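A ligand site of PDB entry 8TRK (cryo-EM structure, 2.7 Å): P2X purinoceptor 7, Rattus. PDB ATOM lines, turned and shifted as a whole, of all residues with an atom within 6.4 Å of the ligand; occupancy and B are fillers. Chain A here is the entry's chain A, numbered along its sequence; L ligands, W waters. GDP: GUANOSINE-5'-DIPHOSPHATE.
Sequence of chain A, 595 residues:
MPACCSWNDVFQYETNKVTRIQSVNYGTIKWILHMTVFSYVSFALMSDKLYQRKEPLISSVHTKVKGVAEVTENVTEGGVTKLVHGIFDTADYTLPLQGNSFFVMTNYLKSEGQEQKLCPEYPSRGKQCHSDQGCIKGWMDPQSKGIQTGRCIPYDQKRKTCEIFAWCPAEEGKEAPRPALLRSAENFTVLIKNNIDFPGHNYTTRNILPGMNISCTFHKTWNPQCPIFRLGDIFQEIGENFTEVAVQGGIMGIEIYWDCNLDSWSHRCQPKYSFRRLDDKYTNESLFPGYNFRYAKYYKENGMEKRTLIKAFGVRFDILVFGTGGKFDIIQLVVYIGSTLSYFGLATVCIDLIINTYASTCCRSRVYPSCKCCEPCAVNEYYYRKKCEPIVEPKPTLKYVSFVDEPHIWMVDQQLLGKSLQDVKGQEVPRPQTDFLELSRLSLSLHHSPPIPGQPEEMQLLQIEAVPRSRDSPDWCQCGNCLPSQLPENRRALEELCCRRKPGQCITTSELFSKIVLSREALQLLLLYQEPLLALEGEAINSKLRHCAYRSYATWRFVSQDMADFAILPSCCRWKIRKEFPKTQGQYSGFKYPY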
ATOM      1  N   GLU A 495      11.811   3.337  -2.737  1.00  0.00           N
ATOM      2  CA  GLU A 495      13.177   3.012  -2.353  1.00  0.00           C
ATOM      3  C   GLU A 495      14.205   4.022  -2.846  1.00  0.00           C
ATOM      4  O   GLU A 495      15.405   3.797  -2.661  1.00  0.00           O
ATOM      5  CB  GLU A 495      13.552   1.623  -2.874  1.00  0.00           C
ATOM      6  CG  GLU A 495      12.512   0.558  -2.646  1.00  0.00           C
ATOM      7  CD  GLU A 495      13.047  -0.835  -2.869  1.00  0.00           C
ATOM      8  OE1 GLU A 495      14.003  -0.997  -3.659  1.00  0.00           O
ATOM      9  OE2 GLU A 495      12.522  -1.780  -2.245  1.00  0.00           O
ATOM     10  N   SER A 543      17.494 -15.208   4.328  1.00  0.00           N
ATOM     11  CA  SER A 543      16.332 -14.312   4.397  1.00  0.00           C
ATOM     12  C   SER A 543      16.086 -13.830   5.815  1.00  0.00           C
ATOM     13  O   SER A 543      15.797 -12.648   6.042  1.00  0.00           O
ATOM     14  CB  SER A 543      15.088 -15.023   3.860  1.00  0.00           C
ATOM     15  OG  SER A 543      14.792 -16.162   4.635  1.00  0.00           O
ATOM     16  N   ARG A 546      18.639 -11.201   6.612  1.00  0.00           N
ATOM     17  CA  ARG A 546      18.354  -9.958   5.900  1.00  0.00           C
ATOM     18  C   ARG A 546      17.246  -9.172   6.598  1.00  0.00           C
ATOM     19  O   ARG A 546      17.361  -7.955   6.802  1.00  0.00           O
ATOM     20  CB  ARG A 546      17.984 -10.270   4.465  1.00  0.00           C
ATOM     21  CG  ARG A 546      17.789  -9.074   3.592  1.00  0.00           C
ATOM     22  CD  ARG A 546      17.837  -9.427   2.137  1.00  0.00           C
ATOM     23  NE  ARG A 546      16.765 -10.346   1.770  1.00  0.00           N
ATOM     24  CZ  ARG A 546      16.916 -11.652   1.591  1.00  0.00           C
ATOM     25  NH1 ARG A 546      18.098 -12.222   1.726  1.00  0.00           N
ATOM     26  NH2 ARG A 546      15.870 -12.390   1.268  1.00  0.00           N
ATOM     27  N   HIS A 547      16.176  -9.866   6.964  1.00  0.00           N
ATOM     28  CA  HIS A 547      15.095  -9.219   7.694  1.00  0.00           C
ATOM     29  C   HIS A 547      15.595  -8.669   9.028  1.00  0.00           C
ATOM     30  O   HIS A 547      15.215  -7.562   9.435  1.00  0.00           O
ATOM     31  CB  HIS A 547      13.937 -10.187   7.901  1.00  0.00           C
ATOM     32  CG  HIS A 547      13.328 -10.683   6.626  1.00  0.00           C
ATOM     33  ND1 HIS A 547      12.163 -11.405   6.593  1.00  0.00           N
ATOM     34  CD2 HIS A 547      13.746 -10.566   5.352  1.00  0.00           C
ATOM     35  CE1 HIS A 547      11.871 -11.700   5.340  1.00  0.00           C
ATOM     36  NE2 HIS A 547      12.811 -11.201   4.569  1.00  0.00           N
ATOM     37  N   TYR A 550      17.471  -5.448   8.440  1.00  0.00           N
ATOM     38  CA  TYR A 550      16.537  -4.338   8.242  1.00  0.00           C
ATOM     39  C   TYR A 550      15.970  -3.870   9.569  1.00  0.00           C
ATOM     40  O   TYR A 550      15.897  -2.668   9.843  1.00  0.00           O
ATOM     41  CB  TYR A 550      15.404  -4.758   7.304  1.00  0.00           C
ATOM     42  CG  TYR A 550      15.805  -5.131   5.895  1.00  0.00           C
ATOM     43  CD1 TYR A 550      16.914  -4.592   5.278  1.00  0.00           C
ATOM     44  CD2 TYR A 550      15.049  -6.034   5.173  1.00  0.00           C
ATOM     45  CE1 TYR A 550      17.251  -4.940   3.988  1.00  0.00           C
ATOM     46  CE2 TYR A 550      15.378  -6.382   3.894  1.00  0.00           C
ATOM     47  CZ  TYR A 550      16.475  -5.837   3.312  1.00  0.00           C
ATOM     48  OH  TYR A 550      16.795  -6.203   2.028  1.00  0.00           O
ATOM     49  N   ALA A 554      16.405  -0.195  11.401  1.00  0.00           N
ATOM     50  CA  ALA A 554      15.223   0.585  11.706  1.00  0.00           C
ATOM     51  C   ALA A 554      15.103   0.882  13.187  1.00  0.00           C
ATOM     52  O   ALA A 554      14.704   1.978  13.582  1.00  0.00           O
ATOM     53  CB  ALA A 554      13.984  -0.125  11.191  1.00  0.00           C
ATOM     54  N   MET A 563       7.629   3.682  14.747  1.00  0.00           N
ATOM     55  CA  MET A 563       8.279   4.245  13.569  1.00  0.00           C
ATOM     56  C   MET A 563       9.167   3.241  12.869  1.00  0.00           C
ATOM     57  O   MET A 563       9.257   3.254  11.642  1.00  0.00           O
ATOM     58  CB  MET A 563       9.079   5.478  13.972  1.00  0.00           C
ATOM     59  CG  MET A 563       8.278   6.497  14.746  1.00  0.00           C
ATOM     60  SD  MET A 563       8.993   8.139  14.739  1.00  0.00           S
ATOM     61  CE  MET A 563      10.602   7.755  15.406  1.00  0.00           C
ATOM     62  N   ALA A 564       9.845   2.374  13.630  1.00  0.00           N
ATOM     63  CA  ALA A 564      10.666   1.347  13.022  1.00  0.00           C
ATOM     64  C   ALA A 564       9.855   0.425  12.126  1.00  0.00           C
ATOM     65  O   ALA A 564      10.386  -0.167  11.183  1.00  0.00           O
ATOM     66  CB  ALA A 564      11.371   0.545  14.104  1.00  0.00           C
ATOM     67  N   ASP A 565       8.567   0.267  12.413  1.00  0.00           N
ATOM     68  CA  ASP A 565       7.704  -0.568  11.573  1.00  0.00           C
ATOM     69  C   ASP A 565       7.474   0.059  10.207  1.00  0.00           C
ATOM     70  O   ASP A 565       7.475  -0.640   9.193  1.00  0.00           O
ATOM     71  CB  ASP A 565       6.379  -0.816  12.279  1.00  0.00           C
ATOM     72  CG  ASP A 565       6.487  -1.812  13.401  1.00  0.00           C
ATOM     73  OD1 ASP A 565       7.570  -2.424  13.558  1.00  0.00           O
ATOM     74  OD2 ASP A 565       5.491  -1.993  14.132  1.00  0.00           O
ATOM     75  N   PHE A 566       7.278   1.369  10.165  1.00  0.00           N
ATOM     76  CA  PHE A 566       6.994   2.093   8.933  1.00  0.00           C
ATOM     77  C   PHE A 566       8.206   2.845   8.398  1.00  0.00           C
ATOM     78  O   PHE A 566       8.083   3.609   7.438  1.00  0.00           O
ATOM     79  CB  PHE A 566       5.834   3.052   9.153  1.00  0.00           C
ATOM     80  CG  PHE A 566       4.527   2.368   9.313  1.00  0.00           C
ATOM     81  CD1 PHE A 566       3.739   2.069   8.217  1.00  0.00           C
ATOM     82  CD2 PHE A 566       4.083   1.985  10.555  1.00  0.00           C
ATOM     83  CE1 PHE A 566       2.545   1.427   8.365  1.00  0.00           C
ATOM     84  CE2 PHE A 566       2.894   1.348  10.715  1.00  0.00           C
ATOM     85  CZ  PHE A 566       2.123   1.067   9.613  1.00  0.00           C
ATOM     86  N   ALA A 567       9.367   2.658   9.005  1.00  0.00           N
ATOM     87  CA  ALA A 567      10.599   3.246   8.516  1.00  0.00           C
ATOM     88  C   ALA A 567      10.835   2.836   7.071  1.00  0.00           C
ATOM     89  O   ALA A 567      10.204   1.929   6.532  1.00  0.00           O
ATOM     90  CB  ALA A 567      11.766   2.810   9.373  1.00  0.00           C
ATOM     91  N   ILE A 568      11.764   3.539   6.429  1.00  0.00           N
ATOM     92  CA  ILE A 568      12.195   3.212   5.077  1.00  0.00           C
ATOM     93  C   ILE A 568      13.713   3.248   5.072  1.00  0.00           C
ATOM     94  O   ILE A 568      14.316   4.271   5.410  1.00  0.00           O
ATOM     95  CB  ILE A 568      11.630   4.181   4.027  1.00  0.00           C
ATOM     96  CG1 ILE A 568      10.115   4.256   4.147  1.00  0.00           C
ATOM     97  CG2 ILE A 568      12.001   3.722   2.641  1.00  0.00           C
ATOM     98  CD1 ILE A 568       9.404   3.003   3.785  1.00  0.00           C
ATOM     99  N   LEU A 569      14.323   2.150   4.696  1.00  0.00           N
ATOM    100  CA  LEU A 569      15.772   2.099   4.632  1.00  0.00           C
ATOM    101  C   LEU A 569      16.278   2.784   3.369  1.00  0.00           C
ATOM    102  O   LEU A 569      15.640   2.699   2.320  1.00  0.00           O
ATOM    103  CB  LEU A 569      16.261   0.659   4.650  1.00  0.00           C
ATOM    104  CG  LEU A 569      16.402  -0.084   5.969  1.00  0.00           C
ATOM    105  CD1 LEU A 569      15.088  -0.423   6.587  1.00  0.00           C
ATOM    106  CD2 LEU A 569      17.175  -1.304   5.656  1.00  0.00           C
ATOM    107  N   PRO A 570      17.420   3.454   3.448  1.00  0.00           N
ATOM    108  CA  PRO A 570      18.026   4.005   2.237  1.00  0.00           C
ATOM    109  C   PRO A 570      18.511   2.910   1.304  1.00  0.00           C
ATOM    110  O   PRO A 570      18.697   1.758   1.681  1.00  0.00           O
ATOM    111  CB  PRO A 570      19.195   4.834   2.767  1.00  0.00           C
ATOM    112  CG  PRO A 570      18.898   5.050   4.188  1.00  0.00           C
ATOM    113  CD  PRO A 570      18.156   3.871   4.644  1.00  0.00           C
ATOM    114  N   ARG A 574      20.184  -0.623   2.403  1.00  0.00           N
ATOM    115  CA  ARG A 574      19.415  -1.754   1.897  1.00  0.00           C
ATOM    116  C   ARG A 574      20.267  -2.649   1.026  1.00  0.00           C
ATOM    117  O   ARG A 574      20.284  -3.874   1.206  1.00  0.00           O
ATOM    118  CB  ARG A 574      18.209  -1.215   1.134  1.00  0.00           C
ATOM    119  CG  ARG A 574      17.439  -2.226   0.341  1.00  0.00           C
ATOM    120  CD  ARG A 574      16.488  -1.561  -0.605  1.00  0.00           C
ATOM    121  NE  ARG A 574      15.705  -0.527   0.067  1.00  0.00           N
ATOM    122  CZ  ARG A 574      14.686  -0.781   0.879  1.00  0.00           C
ATOM    123  NH1 ARG A 574      14.339  -2.023   1.139  1.00  0.00           N
ATOM    124  NH2 ARG A 574      14.030   0.220   1.436  1.00  0.00           N
ATOM    125  N   ARG A 578      21.639  -6.454   1.468  1.00  0.00           N
ATOM    126  CA  ARG A 578      21.312  -7.498   0.497  1.00  0.00           C
ATOM    127  C   ARG A 578      22.560  -8.140  -0.071  1.00  0.00           C
ATOM    128  O   ARG A 578      22.624  -9.354  -0.263  1.00  0.00           O
ATOM    129  CB  ARG A 578      20.436  -6.921  -0.603  1.00  0.00           C
ATOM    130  CG  ARG A 578      18.981  -6.855  -0.234  1.00  0.00           C
ATOM    131  CD  ARG A 578      18.264  -5.723  -0.905  1.00  0.00           C
ATOM    132  NE  ARG A 578      16.860  -5.673  -0.524  1.00  0.00           N
ATOM    133  CZ  ARG A 578      15.900  -5.092  -1.244  1.00  0.00           C
ATOM    134  NH1 ARG A 578      16.188  -4.516  -2.395  1.00  0.00           N
ATOM    135  NH2 ARG A 578      14.658  -5.102  -0.809  1.00  0.00           N
ATOM    136  N   LYS A 583      20.063 -13.168  -2.027  1.00  0.00           N
ATOM    137  CA  LYS A 583      18.989 -14.114  -2.244  1.00  0.00           C
ATOM    138  C   LYS A 583      19.337 -15.019  -3.407  1.00  0.00           C
ATOM    139  O   LYS A 583      19.931 -14.585  -4.394  1.00  0.00           O
ATOM    140  CB  LYS A 583      17.671 -13.398  -2.519  1.00  0.00           C
ATOM    141  CG  LYS A 583      16.454 -14.183  -2.050  1.00  0.00           C
ATOM    142  CD  LYS A 583      15.194 -13.352  -2.062  1.00  0.00           C
ATOM    143  CE  LYS A 583      14.638 -13.204  -3.435  1.00  0.00           C
ATOM    144  NZ  LYS A 583      13.607 -12.157  -3.447  1.00  0.00           N
ATOM    145  N   GLY A 586      15.274 -14.261  -7.500  1.00  0.00           N
ATOM    146  CA  GLY A 586      14.026 -13.551  -7.376  1.00  0.00           C
ATOM    147  C   GLY A 586      14.238 -12.114  -6.927  1.00  0.00           C
ATOM    148  O   GLY A 586      15.254 -11.757  -6.325  1.00  0.00           O
ATOM    149  N   GLN A 587      13.261 -11.269  -7.240  1.00  0.00           N
ATOM    150  CA  GLN A 587      13.325  -9.880  -6.820  1.00  0.00           C
ATOM    151  C   GLN A 587      13.038  -9.782  -5.337  1.00  0.00           C
ATOM    152  O   GLN A 587      12.191 -10.499  -4.801  1.00  0.00           O
ATOM    153  CB  GLN A 587      12.320  -9.009  -7.581  1.00  0.00           C
ATOM    154  CG  GLN A 587      12.095  -9.297  -9.049  1.00  0.00           C
ATOM    155  CD  GLN A 587      13.361  -9.271  -9.874  1.00  0.00           C
ATOM    156  OE1 GLN A 587      13.934  -8.210 -10.118  1.00  0.00           O
ATOM    157  NE2 GLN A 587      13.768 -10.430 -10.367  1.00  0.00           N
ATOM    158  N   TYR A 588      13.760  -8.880  -4.667  1.00  0.00           N
ATOM    159  CA  TYR A 588      13.449  -8.537  -3.295  1.00  0.00           C
ATOM    160  C   TYR A 588      12.108  -7.811  -3.224  1.00  0.00           C
ATOM    161  O   TYR A 588      11.870  -6.850  -3.956  1.00  0.00           O
ATOM    162  CB  TYR A 588      14.563  -7.668  -2.736  1.00  0.00           C
ATOM    163  CG  TYR A 588      15.898  -8.365  -2.678  1.00  0.00           C
ATOM    164  CD1 TYR A 588      16.167  -9.317  -1.710  1.00  0.00           C
ATOM    165  CD2 TYR A 588      16.884  -8.079  -3.605  1.00  0.00           C
ATOM    166  CE1 TYR A 588      17.381  -9.934  -1.648  1.00  0.00           C
ATOM    167  CE2 TYR A 588      18.102  -8.706  -3.557  1.00  0.00           C
ATOM    168  CZ  TYR A 588      18.343  -9.626  -2.575  1.00  0.00           C
ATOM    169  OH  TYR A 588      19.570 -10.256  -2.530  1.00  0.00           O
ATOM    170  N   SER A 589      11.230  -8.277  -2.328  1.00  0.00           N
ATOM    171  CA  SER A 589       9.891  -7.715  -2.253  1.00  0.00           C
ATOM    172  C   SER A 589       9.897  -6.248  -1.844  1.00  0.00           C
ATOM    173  O   SER A 589       9.052  -5.466  -2.295  1.00  0.00           O
ATOM    174  CB  SER A 589       9.041  -8.534  -1.274  1.00  0.00           C
ATOM    175  OG  SER A 589       8.933  -9.868  -1.693  1.00  0.00           O
ATOM    176  N   GLY A 590      10.839  -5.846  -0.997  1.00  0.00           N
ATOM    177  CA  GLY A 590      10.852  -4.503  -0.473  1.00  0.00           C
ATOM    178  C   GLY A 590       9.892  -4.321   0.676  1.00  0.00           C
ATOM    179  O   GLY A 590       9.353  -5.279   1.254  1.00  0.00           O
ATOM    180  N   PHE A 591       9.684  -3.059   1.034  1.00  0.00           N
ATOM    181  CA  PHE A 591       8.794  -2.736   2.146  1.00  0.00           C
ATOM    182  C   PHE A 591       7.404  -3.281   1.903  1.00  0.00           C
ATOM    183  O   PHE A 591       6.812  -3.082   0.839  1.00  0.00           O
ATOM    184  CB  PHE A 591       8.732  -1.230   2.360  1.00  0.00           C
ATOM    185  CG  PHE A 591       7.925  -0.822   3.551  1.00  0.00           C
ATOM    186  CD1 PHE A 591       8.264  -1.234   4.809  1.00  0.00           C
ATOM    187  CD2 PHE A 591       6.797  -0.032   3.408  1.00  0.00           C
ATOM    188  CE1 PHE A 591       7.529  -0.873   5.904  1.00  0.00           C
ATOM    189  CE2 PHE A 591       6.062   0.328   4.503  1.00  0.00           C
ATOM    190  CZ  PHE A 591       6.427  -0.091   5.746  1.00  0.00           C
ATOM    191  N   LYS A 592       6.866  -3.968   2.911  1.00  0.00           N
ATOM    192  CA  LYS A 592       5.530  -4.516   2.878  1.00  0.00           C
ATOM    193  C   LYS A 592       4.733  -3.970   4.055  1.00  0.00           C
ATOM    194  O   LYS A 592       5.220  -3.946   5.186  1.00  0.00           O
ATOM    195  CB  LYS A 592       5.554  -6.050   2.901  1.00  0.00           C
ATOM    196  CG  LYS A 592       4.212  -6.709   2.688  1.00  0.00           C
ATOM    197  CD  LYS A 592       3.512  -6.951   4.008  1.00  0.00           C
ATOM    198  CE  LYS A 592       2.194  -7.679   3.833  1.00  0.00           C
ATOM    199  NZ  LYS A 592       1.530  -7.853   5.143  1.00  0.00           N
ATOM    200  N   TYR A 593       3.521  -3.534   3.777  1.00  0.00           N
ATOM    201  CA  TYR A 593       2.667  -2.898   4.767  1.00  0.00           C
ATOM    202  C   TYR A 593       2.436  -3.816   5.959  1.00  0.00           C
ATOM    203  O   TYR A 593       1.931  -4.932   5.794  1.00  0.00           O
ATOM    204  CB  TYR A 593       1.346  -2.539   4.115  1.00  0.00           C
ATOM    205  CG  TYR A 593       0.356  -1.867   5.019  1.00  0.00           C
ATOM    206  CD1 TYR A 593       0.698  -0.725   5.715  1.00  0.00           C
ATOM    207  CD2 TYR A 593      -0.932  -2.356   5.154  1.00  0.00           C
ATOM    208  CE1 TYR A 593      -0.208  -0.102   6.543  1.00  0.00           C
ATOM    209  CE2 TYR A 593      -1.841  -1.741   5.979  1.00  0.00           C
ATOM    210  CZ  TYR A 593      -1.473  -0.611   6.669  1.00  0.00           C
ATOM    211  OH  TYR A 593      -2.386  -0.005   7.491  1.00  0.00           O
HETATM  212  PB  GDP L   1      12.232 -10.970  -0.069  1.00  0.00           P
HETATM  213  O1B GDP L   1      13.318 -11.148  -1.097  1.00  0.00           O
HETATM  214  O2B GDP L   1      11.000 -11.735  -0.498  1.00  0.00           O
HETATM  215  O3B GDP L   1      12.697 -11.491   1.269  1.00  0.00           O
HETATM  216  O3A GDP L   1      11.863  -9.418   0.064  1.00  0.00           O
HETATM  217  PA  GDP L   1      12.706  -8.456   1.037  1.00  0.00           P
HETATM  218  O1A GDP L   1      13.978  -9.109   1.498  1.00  0.00           O
HETATM  219  O2A GDP L   1      13.019  -7.127   0.395  1.00  0.00           O
HETATM  220  O5' GDP L   1      11.688  -8.254   2.240  1.00  0.00           O
HETATM  221  C5' GDP L   1      12.248  -7.926   3.499  1.00  0.00           C
HETATM  222  C4' GDP L   1      11.231  -7.661   4.587  1.00  0.00           C
HETATM  223  O4' GDP L   1      11.748  -6.578   5.347  1.00  0.00           O
HETATM  224  C3' GDP L   1       9.852  -7.280   4.086  1.00  0.00           C
HETATM  225  O3' GDP L   1       8.900  -8.240   4.528  1.00  0.00           O
HETATM  226  C2' GDP L   1       9.567  -5.922   4.676  1.00  0.00           C
HETATM  227  O2' GDP L   1       8.502  -6.005   5.628  1.00  0.00           O
HETATM  228  C1' GDP L   1      10.842  -5.489   5.375  1.00  0.00           C
HETATM  229  N9  GDP L   1      11.459  -4.315   4.700  1.00  0.00           N
HETATM  230  C8  GDP L   1      12.078  -4.287   3.510  1.00  0.00           C
HETATM  231  N7  GDP L   1      12.517  -3.042   3.214  1.00  0.00           N
HETATM  232  C5  GDP L   1      12.171  -2.252   4.239  1.00  0.00           C
HETATM  233  C6  GDP L   1      12.316  -0.839   4.577  1.00  0.00           C
HETATM  234  O6  GDP L   1      12.898  -0.052   3.795  1.00  0.00           O
HETATM  235  N1  GDP L   1      11.817  -0.419   5.743  1.00  0.00           N
HETATM  236  C2  GDP L   1      11.200  -1.245   6.588  1.00  0.00           C
HETATM  237  N2  GDP L   1      10.723  -0.738   7.742  1.00  0.00           N
HETATM  238  N3  GDP L   1      11.017  -2.559   6.352  1.00  0.00           N
HETATM  239  C4  GDP L   1      11.484  -3.099   5.208  1.00  0.00           C
HETATM  240  O   HOH W   1       9.132 -11.214   2.016  1.00  0.00           O
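The backbone NH (N) of Lys 583 lies within hydrogen-bond range of the side-chain hydroxyl (OH) of Tyr 588, at 3.0 Å. The side-chain amino group (NZ) of Lys 583 is in hydrogen-bond range of the backbone carbonyl oxygen (O) of Gln 587 (2.6 Å). O of Gly 586 sits close to NZ of Lys 583 (3.3 Å). The backbone carbonyl oxygen (O) of Leu 569 sits at hydrogen-bond distance from the guanidinium group (NH2) of Arg 574, 3.1 Å away. The side-chain carboxylate (OE2) of Glu 495 is in salt-bridge range of the guanidinium group (NH1) of Arg 574 (3.8 Å). The guanidinium group (NE) of Arg 578 is in hydrogen-bond range of the side-chain hydroxyl (OH) of Tyr 550, at 2.6 Å.
NZ of Lys 583 is in salt-bridge range of O1B of the ligand, 2.6 Å away. The guanidinium group (NH2) of Arg 574 lies within hydrogen-bond range of an oxygen (O6) of the ligand (2.6 Å). The backbone NH of Ser 589 sits at hydrogen-bond distance from an oxygen (O3A) of the ligand (2.7 Å). An oxygen (O2B) of the ligand is in hydrogen-bond range of the side-chain hydroxyl of Ser 589, 3.0 Å away. The backbone NH of Leu 569 sits at hydrogen-bond distance from an oxygen (O6) of the ligand. O2A of the ligand is in salt-bridge range of NH2 of Arg 578 (2.9 Å). The backbone NH (N) of Gly 590 is in hydrogen-bond range of an oxygen (O2A) of the ligand (2.9 Å). A nitrogen (N1) of the ligand lies within hydrogen-bond range of the backbone carbonyl oxygen (O) of Ala 567, at 3.0 Å. The guanidinium group of Arg 546 lies within salt-bridge range of an oxygen (O1A) of the ligand, 3.1 Å away. NE2 of His 547 sits at hydrogen-bond distance from O3B of the ligand (3.3 Å).
Residues that only touch the ligand: Tyr 550, Tyr 588, Phe 591, Ala 564, Asp 565, Ile 568, Lys 592 and Gln 587. 17 residues have an atom within 4 Å of the ligand: Arg 546, His 547, Tyr 550, Ala 564, Asp 565, Ala 567, Ile 568, Leu 569, Arg 574, Arg 578, Lys 583, Gln 587, Tyr 588, Ser 589, Gly 590, Phe 591 and Lys 592.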
